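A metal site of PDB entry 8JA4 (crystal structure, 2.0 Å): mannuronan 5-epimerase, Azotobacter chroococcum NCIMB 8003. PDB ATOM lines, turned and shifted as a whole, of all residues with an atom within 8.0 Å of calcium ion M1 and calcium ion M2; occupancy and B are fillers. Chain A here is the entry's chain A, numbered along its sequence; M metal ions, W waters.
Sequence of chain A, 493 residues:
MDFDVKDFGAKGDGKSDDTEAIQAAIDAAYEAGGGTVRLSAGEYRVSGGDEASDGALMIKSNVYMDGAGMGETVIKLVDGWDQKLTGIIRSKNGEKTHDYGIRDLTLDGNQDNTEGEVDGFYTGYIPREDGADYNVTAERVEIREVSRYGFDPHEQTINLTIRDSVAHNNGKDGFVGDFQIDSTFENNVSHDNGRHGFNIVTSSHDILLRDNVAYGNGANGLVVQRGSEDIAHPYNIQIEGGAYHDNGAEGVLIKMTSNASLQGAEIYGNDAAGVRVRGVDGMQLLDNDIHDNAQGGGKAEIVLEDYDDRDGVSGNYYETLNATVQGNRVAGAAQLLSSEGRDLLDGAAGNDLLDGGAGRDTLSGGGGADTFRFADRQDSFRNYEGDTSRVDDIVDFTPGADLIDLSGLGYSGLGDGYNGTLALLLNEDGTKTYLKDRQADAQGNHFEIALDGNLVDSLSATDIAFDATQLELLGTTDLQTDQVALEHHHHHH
O of Asp 370 sits at hydrogen-bond distance from N of Leu 403 (2.8 Å). The side-chain carboxylate (OD2) of Asp 402 lies within hydrogen-bond range of the backbone NH (N) of Thr 398 (2.9 Å). N of Ala 334 is in hydrogen-bond range of OD1 of Asp 352, 2.7 Å away. OD2 of Asp 396 is in hydrogen-bond range of N of Gly 366. OD1 of Asp 396 is in hydrogen-bond range of N of Gly 365. The backbone NH (N) of Thr 371 is in hydrogen-bond range of the backbone carbonyl oxygen (O) of Asp 352, 2.9 Å away.
Within 4 Å of calcium ion M1: Ala 348, Gly 350, Asp 352, Gly 365, Gly 366, Gly 367 and Asp 370. The nearest printed residue that does not touch calcium ion M1 is Ala 349 (4.2 Å).
Five residues have an atom within 4 Å of calcium ion M2: Gly 366, Gly 367, Gly 368, Asp 370 and Asp 402.
The backbone carbonyl oxygen (O) of Gly 365 binds calcium ion M1 (2.2 Å). The side-chain carboxylate (OD2) of Asp 370 is bound to calcium ion M1. Calcium ion M1 is bound by O of Ala 348 (2.3 Å). OD2 of Asp 352 binds calcium ion M1 (2.4 Å). The backbone carbonyl oxygen (O) of Gly 350 is bound to calcium ion M1 (2.4 Å). Calcium ion M1 is bound by the backbone carbonyl oxygen (O) of Gly 367, 2.4 Å away. OD1 of Asp 370 binds calcium ion M1. Calcium ion M1 has seven donor atoms within binding distance.
Calcium ion M2 is bound by O of Gly 366 (2.4 Å), OD1 of Asp 370 (2.4 Å), OD1 of Asp 402 (2.5 Å), O of Gly 368 (2.5 Å), water W2 (2.6 Å) and water W1 (2.6 Å).
Water W2 lies within hydrogen-bond range of OD2 of Asp 402 (2.6 Å) and O of Asp 396 (3.1 Å).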
ATOM      1  N   VAL A 330     -22.409   6.632  17.518  1.00  0.00           N
ATOM      2  CA  VAL A 330     -21.009   6.852  17.166  1.00  0.00           C
ATOM      3  C   VAL A 330     -20.612   5.895  16.069  1.00  0.00           C
ATOM      4  O   VAL A 330     -20.367   4.705  16.329  1.00  0.00           O
ATOM      5  CB  VAL A 330     -20.058   6.678  18.359  1.00  0.00           C
ATOM      6  CG1 VAL A 330     -18.621   6.976  17.919  1.00  0.00           C
ATOM      7  CG2 VAL A 330     -20.468   7.603  19.511  1.00  0.00           C
ATOM      8  N   GLY A 332     -18.086   4.715  14.410  1.00  0.00           N
ATOM      9  CA  GLY A 332     -16.646   4.554  14.387  1.00  0.00           C
ATOM     10  C   GLY A 332     -16.103   4.404  15.807  1.00  0.00           C
ATOM     11  O   GLY A 332     -16.836   4.333  16.779  1.00  0.00           O
ATOM     12  N   ALA A 333     -14.796   4.346  15.894  1.00  0.00           N
ATOM     13  CA  ALA A 333     -14.175   3.870  17.136  1.00  0.00           C
ATOM     14  C   ALA A 333     -14.210   4.942  18.229  1.00  0.00           C
ATOM     15  O   ALA A 333     -13.903   6.127  17.993  1.00  0.00           O
ATOM     16  CB  ALA A 333     -12.736   3.476  16.856  1.00  0.00           C
ATOM     17  N   ALA A 334     -14.534   4.535  19.456  1.00  0.00           N
ATOM     18  CA  ALA A 334     -14.367   5.435  20.602  1.00  0.00           C
ATOM     19  C   ALA A 334     -13.212   4.969  21.491  1.00  0.00           C
ATOM     20  O   ALA A 334     -13.136   3.784  21.857  1.00  0.00           O
ATOM     21  CB  ALA A 334     -15.673   5.545  21.395  1.00  0.00           C
ATOM     22  N   ASP A 346     -19.621   4.108  28.023  1.00  0.00           N
ATOM     23  CA  ASP A 346     -20.376   3.292  27.062  1.00  0.00           C
ATOM     24  C   ASP A 346     -19.849   3.558  25.665  1.00  0.00           C
ATOM     25  O   ASP A 346     -19.920   4.692  25.181  1.00  0.00           O
ATOM     26  CB  ASP A 346     -21.860   3.641  27.092  1.00  0.00           C
ATOM     27  CG  ASP A 346     -22.561   3.262  28.397  1.00  0.00           C
ATOM     28  OD1 ASP A 346     -22.000   2.479  29.203  1.00  0.00           O
ATOM     29  OD2 ASP A 346     -23.702   3.754  28.600  1.00  0.00           O
ATOM     30  N   GLY A 347     -19.367   2.507  24.998  1.00  0.00           N
ATOM     31  CA  GLY A 347     -19.141   2.546  23.567  1.00  0.00           C
ATOM     32  C   GLY A 347     -20.450   2.493  22.760  1.00  0.00           C
ATOM     33  O   GLY A 347     -21.564   2.477  23.288  1.00  0.00           O
ATOM     34  N   ALA A 348     -20.291   2.450  21.428  1.00  0.00           N
ATOM     35  CA  ALA A 348     -21.388   2.585  20.486  1.00  0.00           C
ATOM     36  C   ALA A 348     -21.083   1.592  19.389  1.00  0.00           C
ATOM     37  O   ALA A 348     -20.429   0.575  19.665  1.00  0.00           O
ATOM     38  CB  ALA A 348     -21.530   4.016  19.972  1.00  0.00           C
ATOM     39  N   ALA A 349     -21.569   1.821  18.165  1.00  0.00           N
ATOM     40  CA  ALA A 349     -21.490   0.784  17.127  1.00  0.00           C
ATOM     41  C   ALA A 349     -20.074   0.484  16.653  1.00  0.00           C
ATOM     42  O   ALA A 349     -19.893  -0.511  15.938  1.00  0.00           O
ATOM     43  CB  ALA A 349     -22.341   1.195  15.913  1.00  0.00           C
ATOM     44  N   GLY A 350     -19.072   1.302  17.015  1.00  0.00           N
ATOM     45  CA  GLY A 350     -17.692   1.080  16.613  1.00  0.00           C
ATOM     46  C   GLY A 350     -16.959   0.010  17.432  1.00  0.00           C
ATOM     47  O   GLY A 350     -17.488  -0.559  18.385  1.00  0.00           O
ATOM     48  N   ASN A 351     -15.740  -0.296  17.004  1.00  0.00           N
ATOM     49  CA  ASN A 351     -14.841  -1.210  17.717  1.00  0.00           C
ATOM     50  C   ASN A 351     -14.067  -0.351  18.704  1.00  0.00           C
ATOM     51  O   ASN A 351     -13.089   0.302  18.346  1.00  0.00           O
ATOM     52  CB  ASN A 351     -13.897  -1.913  16.751  1.00  0.00           C
ATOM     53  CG  ASN A 351     -14.571  -2.927  15.843  1.00  0.00           C
ATOM     54  OD1 ASN A 351     -15.749  -3.281  15.984  1.00  0.00           O
ATOM     55  ND2 ASN A 351     -13.800  -3.382  14.879  1.00  0.00           N
ATOM     56  N   ASP A 352     -14.531  -0.299  19.948  1.00  0.00           N
ATOM     57  CA  ASP A 352     -14.062   0.684  20.914  1.00  0.00           C
ATOM     58  C   ASP A 352     -13.035   0.118  21.880  1.00  0.00           C
ATOM     59  O   ASP A 352     -12.946  -1.088  22.133  1.00  0.00           O
ATOM     60  CB  ASP A 352     -15.256   1.229  21.703  1.00  0.00           C
ATOM     61  CG  ASP A 352     -16.422   1.662  20.785  1.00  0.00           C
ATOM     62  OD1 ASP A 352     -16.236   2.473  19.830  1.00  0.00           O
ATOM     63  OD2 ASP A 352     -17.547   1.195  21.032  1.00  0.00           O
ATOM     64  N   LEU A 353     -12.264   1.020  22.473  1.00  0.00           N
ATOM     65  CA  LEU A 353     -11.317   0.678  23.517  1.00  0.00           C
ATOM     66  C   LEU A 353     -11.790   1.332  24.809  1.00  0.00           C
ATOM     67  O   LEU A 353     -11.883   2.577  24.876  1.00  0.00           O
ATOM     68  CB  LEU A 353      -9.911   1.169  23.156  1.00  0.00           C
ATOM     69  CG  LEU A 353      -8.876   1.099  24.284  1.00  0.00           C
ATOM     70  CD1 LEU A 353      -8.700  -0.364  24.606  1.00  0.00           C
ATOM     71  CD2 LEU A 353      -7.526   1.684  23.839  1.00  0.00           C
ATOM     72  N   LEU A 354     -12.048   0.531  25.845  1.00  0.00           N
ATOM     73  CA  LEU A 354     -12.554   1.027  27.126  1.00  0.00           C
ATOM     74  C   LEU A 354     -11.610   0.685  28.254  1.00  0.00           C
ATOM     75  O   LEU A 354     -11.225  -0.487  28.398  1.00  0.00           O
ATOM     76  CB  LEU A 354     -13.939   0.443  27.424  1.00  0.00           C
ATOM     77  CG  LEU A 354     -14.965   0.958  26.452  1.00  0.00           C
ATOM     78  CD1 LEU A 354     -15.137  -0.085  25.372  1.00  0.00           C
ATOM     79  CD2 LEU A 354     -16.217   1.124  27.272  1.00  0.00           C
ATOM     80  N   SER A 364     -19.501  -0.483  29.016  1.00  0.00           N
ATOM     81  CA  SER A 364     -20.248  -1.287  28.053  1.00  0.00           C
ATOM     82  C   SER A 364     -19.744  -0.981  26.662  1.00  0.00           C
ATOM     83  O   SER A 364     -19.332   0.150  26.385  1.00  0.00           O
ATOM     84  CB  SER A 364     -21.742  -1.030  28.184  1.00  0.00           C
ATOM     85  OG  SER A 364     -22.088   0.116  27.463  1.00  0.00           O
ATOM     86  N   GLY A 365     -19.676  -2.001  25.805  1.00  0.00           N
ATOM     87  CA  GLY A 365     -19.108  -1.777  24.495  1.00  0.00           C
ATOM     88  C   GLY A 365     -20.114  -1.432  23.407  1.00  0.00           C
ATOM     89  O   GLY A 365     -19.763  -0.820  22.377  1.00  0.00           O
ATOM     90  N   GLY A 366     -21.362  -1.842  23.603  1.00  0.00           N
ATOM     91  CA  GLY A 366     -22.313  -1.729  22.485  1.00  0.00           C
ATOM     92  C   GLY A 366     -21.933  -2.673  21.353  1.00  0.00           C
ATOM     93  O   GLY A 366     -21.207  -3.676  21.543  1.00  0.00           O
ATOM     94  N   GLY A 367     -22.428  -2.344  20.144  1.00  0.00           N
ATOM     95  CA  GLY A 367     -22.203  -3.199  18.985  1.00  0.00           C
ATOM     96  C   GLY A 367     -20.745  -3.154  18.564  1.00  0.00           C
ATOM     97  O   GLY A 367     -19.923  -2.466  19.163  1.00  0.00           O
ATOM     98  N   GLY A 368     -20.373  -3.968  17.566  1.00  0.00           N
ATOM     99  CA  GLY A 368     -18.962  -4.075  17.203  1.00  0.00           C
ATOM    100  C   GLY A 368     -18.151  -4.889  18.205  1.00  0.00           C
ATOM    101  O   GLY A 368     -18.649  -5.400  19.206  1.00  0.00           O
ATOM    102  N   ALA A 369     -16.851  -5.000  17.951  1.00  0.00           N
ATOM    103  CA  ALA A 369     -15.967  -5.805  18.796  1.00  0.00           C
ATOM    104  C   ALA A 369     -15.121  -4.851  19.629  1.00  0.00           C
ATOM    105  O   ALA A 369     -14.296  -4.107  19.093  1.00  0.00           O
ATOM    106  CB  ALA A 369     -15.056  -6.707  17.955  1.00  0.00           C
ATOM    107  N   ASP A 370     -15.321  -4.879  20.945  1.00  0.00           N
ATOM    108  CA  ASP A 370     -14.708  -3.900  21.825  1.00  0.00           C
ATOM    109  C   ASP A 370     -13.676  -4.555  22.743  1.00  0.00           C
ATOM    110  O   ASP A 370     -13.802  -5.719  23.142  1.00  0.00           O
ATOM    111  CB  ASP A 370     -15.768  -3.191  22.675  1.00  0.00           C
ATOM    112  CG  ASP A 370     -16.913  -2.640  21.820  1.00  0.00           C
ATOM    113  OD1 ASP A 370     -18.021  -3.146  21.917  1.00  0.00           O
ATOM    114  OD2 ASP A 370     -16.721  -1.693  21.070  1.00  0.00           O
ATOM    115  N   THR A 371     -12.664  -3.771  23.086  1.00  0.00           N
ATOM    116  CA  THR A 371     -11.611  -4.205  23.991  1.00  0.00           C
ATOM    117  C   THR A 371     -11.760  -3.473  25.315  1.00  0.00           C
ATOM    118  O   THR A 371     -11.695  -2.236  25.364  1.00  0.00           O
ATOM    119  CB  THR A 371     -10.240  -3.960  23.372  1.00  0.00           C
ATOM    120  OG1 THR A 371     -10.124  -4.750  22.167  1.00  0.00           O
ATOM    121  CG2 THR A 371      -9.170  -4.379  24.323  1.00  0.00           C
ATOM    122  N   PHE A 372     -12.021  -4.243  26.378  1.00  0.00           N
ATOM    123  CA  PHE A 372     -12.052  -3.687  27.730  1.00  0.00           C
ATOM    124  C   PHE A 372     -10.685  -3.956  28.351  1.00  0.00           C
ATOM    125  O   PHE A 372     -10.357  -5.107  28.687  1.00  0.00           O
ATOM    126  CB  PHE A 372     -13.155  -4.345  28.538  1.00  0.00           C
ATOM    127  CG  PHE A 372     -14.512  -4.266  27.913  1.00  0.00           C
ATOM    128  CD1 PHE A 372     -15.401  -3.239  28.257  1.00  0.00           C
ATOM    129  CD2 PHE A 372     -14.929  -5.230  26.990  1.00  0.00           C
ATOM    130  CE1 PHE A 372     -16.673  -3.192  27.697  1.00  0.00           C
ATOM    131  CE2 PHE A 372     -16.187  -5.184  26.432  1.00  0.00           C
ATOM    132  CZ  PHE A 372     -17.069  -4.158  26.783  1.00  0.00           C
ATOM    133  N   ASP A 396     -22.148  -5.688  29.037  1.00  0.00           N
ATOM    134  CA  ASP A 396     -22.633  -6.423  27.869  1.00  0.00           C
ATOM    135  C   ASP A 396     -21.528  -7.200  27.202  1.00  0.00           C
ATOM    136  O   ASP A 396     -21.436  -7.223  25.977  1.00  0.00           O
ATOM    137  CB  ASP A 396     -23.229  -5.469  26.836  1.00  0.00           C
ATOM    138  CG  ASP A 396     -22.179  -4.440  26.311  1.00  0.00           C
ATOM    139  OD1 ASP A 396     -21.078  -4.270  26.928  1.00  0.00           O
ATOM    140  OD2 ASP A 396     -22.424  -3.810  25.272  1.00  0.00           O
ATOM    141  N   PHE A 397     -20.643  -7.836  27.968  1.00  0.00           N
ATOM    142  CA  PHE A 397     -19.567  -8.552  27.306  1.00  0.00           C
ATOM    143  C   PHE A 397     -20.131  -9.660  26.435  1.00  0.00           C
ATOM    144  O   PHE A 397     -20.974 -10.431  26.868  1.00  0.00           O
ATOM    145  CB  PHE A 397     -18.586  -9.143  28.304  1.00  0.00           C
ATOM    146  CG  PHE A 397     -17.335  -9.662  27.653  1.00  0.00           C
ATOM    147  CD1 PHE A 397     -17.237 -11.003  27.276  1.00  0.00           C
ATOM    148  CD2 PHE A 397     -16.256  -8.823  27.407  1.00  0.00           C
ATOM    149  CE1 PHE A 397     -16.083 -11.479  26.670  1.00  0.00           C
ATOM    150  CE2 PHE A 397     -15.103  -9.290  26.804  1.00  0.00           C
ATOM    151  CZ  PHE A 397     -15.026 -10.643  26.428  1.00  0.00           C
ATOM    152  N   THR A 398     -19.619  -9.748  25.205  1.00  0.00           N
ATOM    153  CA  THR A 398     -20.180 -10.621  24.166  1.00  0.00           C
ATOM    154  C   THR A 398     -19.112 -11.616  23.731  1.00  0.00           C
ATOM    155  O   THR A 398     -18.166 -11.248  23.017  1.00  0.00           O
ATOM    156  CB  THR A 398     -20.654  -9.768  22.992  1.00  0.00           C
ATOM    157  OG1 THR A 398     -21.452  -8.685  23.481  1.00  0.00           O
ATOM    158  CG2 THR A 398     -21.480 -10.584  22.024  1.00  0.00           C
ATOM    159  N   ALA A 401     -16.856 -11.886  20.233  1.00  0.00           N
ATOM    160  CA  ALA A 401     -16.673 -10.572  19.616  1.00  0.00           C
ATOM    161  C   ALA A 401     -15.793  -9.653  20.461  1.00  0.00           C
ATOM    162  O   ALA A 401     -14.781  -9.118  19.993  1.00  0.00           O
ATOM    163  CB  ALA A 401     -18.045  -9.909  19.367  1.00  0.00           C
ATOM    164  N   ASP A 402     -16.174  -9.431  21.718  1.00  0.00           N
ATOM    165  CA  ASP A 402     -15.400  -8.549  22.562  1.00  0.00           C
ATOM    166  C   ASP A 402     -14.141  -9.257  23.086  1.00  0.00           C
ATOM    167  O   ASP A 402     -13.988 -10.486  22.987  1.00  0.00           O
ATOM    168  CB  ASP A 402     -16.262  -8.062  23.712  1.00  0.00           C
ATOM    169  CG  ASP A 402     -17.464  -7.281  23.259  1.00  0.00           C
ATOM    170  OD1 ASP A 402     -17.378  -6.515  22.239  1.00  0.00           O
ATOM    171  OD2 ASP A 402     -18.502  -7.431  23.949  1.00  0.00           O
ATOM    172  N   LEU A 403     -13.258  -8.453  23.698  1.00  0.00           N
ATOM    173  CA  LEU A 403     -12.005  -8.932  24.264  1.00  0.00           C
ATOM    174  C   LEU A 403     -11.758  -8.262  25.605  1.00  0.00           C
ATOM    175  O   LEU A 403     -11.972  -7.063  25.747  1.00  0.00           O
ATOM    176  CB  LEU A 403     -10.803  -8.624  23.347  1.00  0.00           C
ATOM    177  CG  LEU A 403      -9.415  -9.090  23.841  1.00  0.00           C
ATOM    178  CD1 LEU A 403      -9.241 -10.620  23.773  1.00  0.00           C
ATOM    179  CD2 LEU A 403      -8.357  -8.415  22.983  1.00  0.00           C
ATOM    180  N   THR A 476      -9.110  -6.091  19.197  1.00  0.00           N
ATOM    181  CA  THR A 476     -10.223  -5.775  18.315  1.00  0.00           C
ATOM    182  C   THR A 476     -10.170  -4.369  17.720  1.00  0.00           C
ATOM    183  O   THR A 476     -11.035  -4.005  16.912  1.00  0.00           O
ATOM    184  CB  THR A 476     -11.548  -5.942  19.045  1.00  0.00           C
ATOM    185  OG1 THR A 476     -11.767  -4.818  19.920  1.00  0.00           O
ATOM    186  CG2 THR A 476     -11.547  -7.249  19.806  1.00  0.00           C
HETATM  187 CA    CA M   1     -18.708  -0.772  20.432  1.00  0.00          CA
HETATM  188 CA    CA M   2     -19.341  -5.103  21.609  1.00  0.00          CA
HETATM  189  O   HOH W   1     -20.917  -7.070  20.960  1.00  0.00           O
HETATM  190  O   HOH W   2     -19.811  -5.239  24.165  1.00  0.00           O
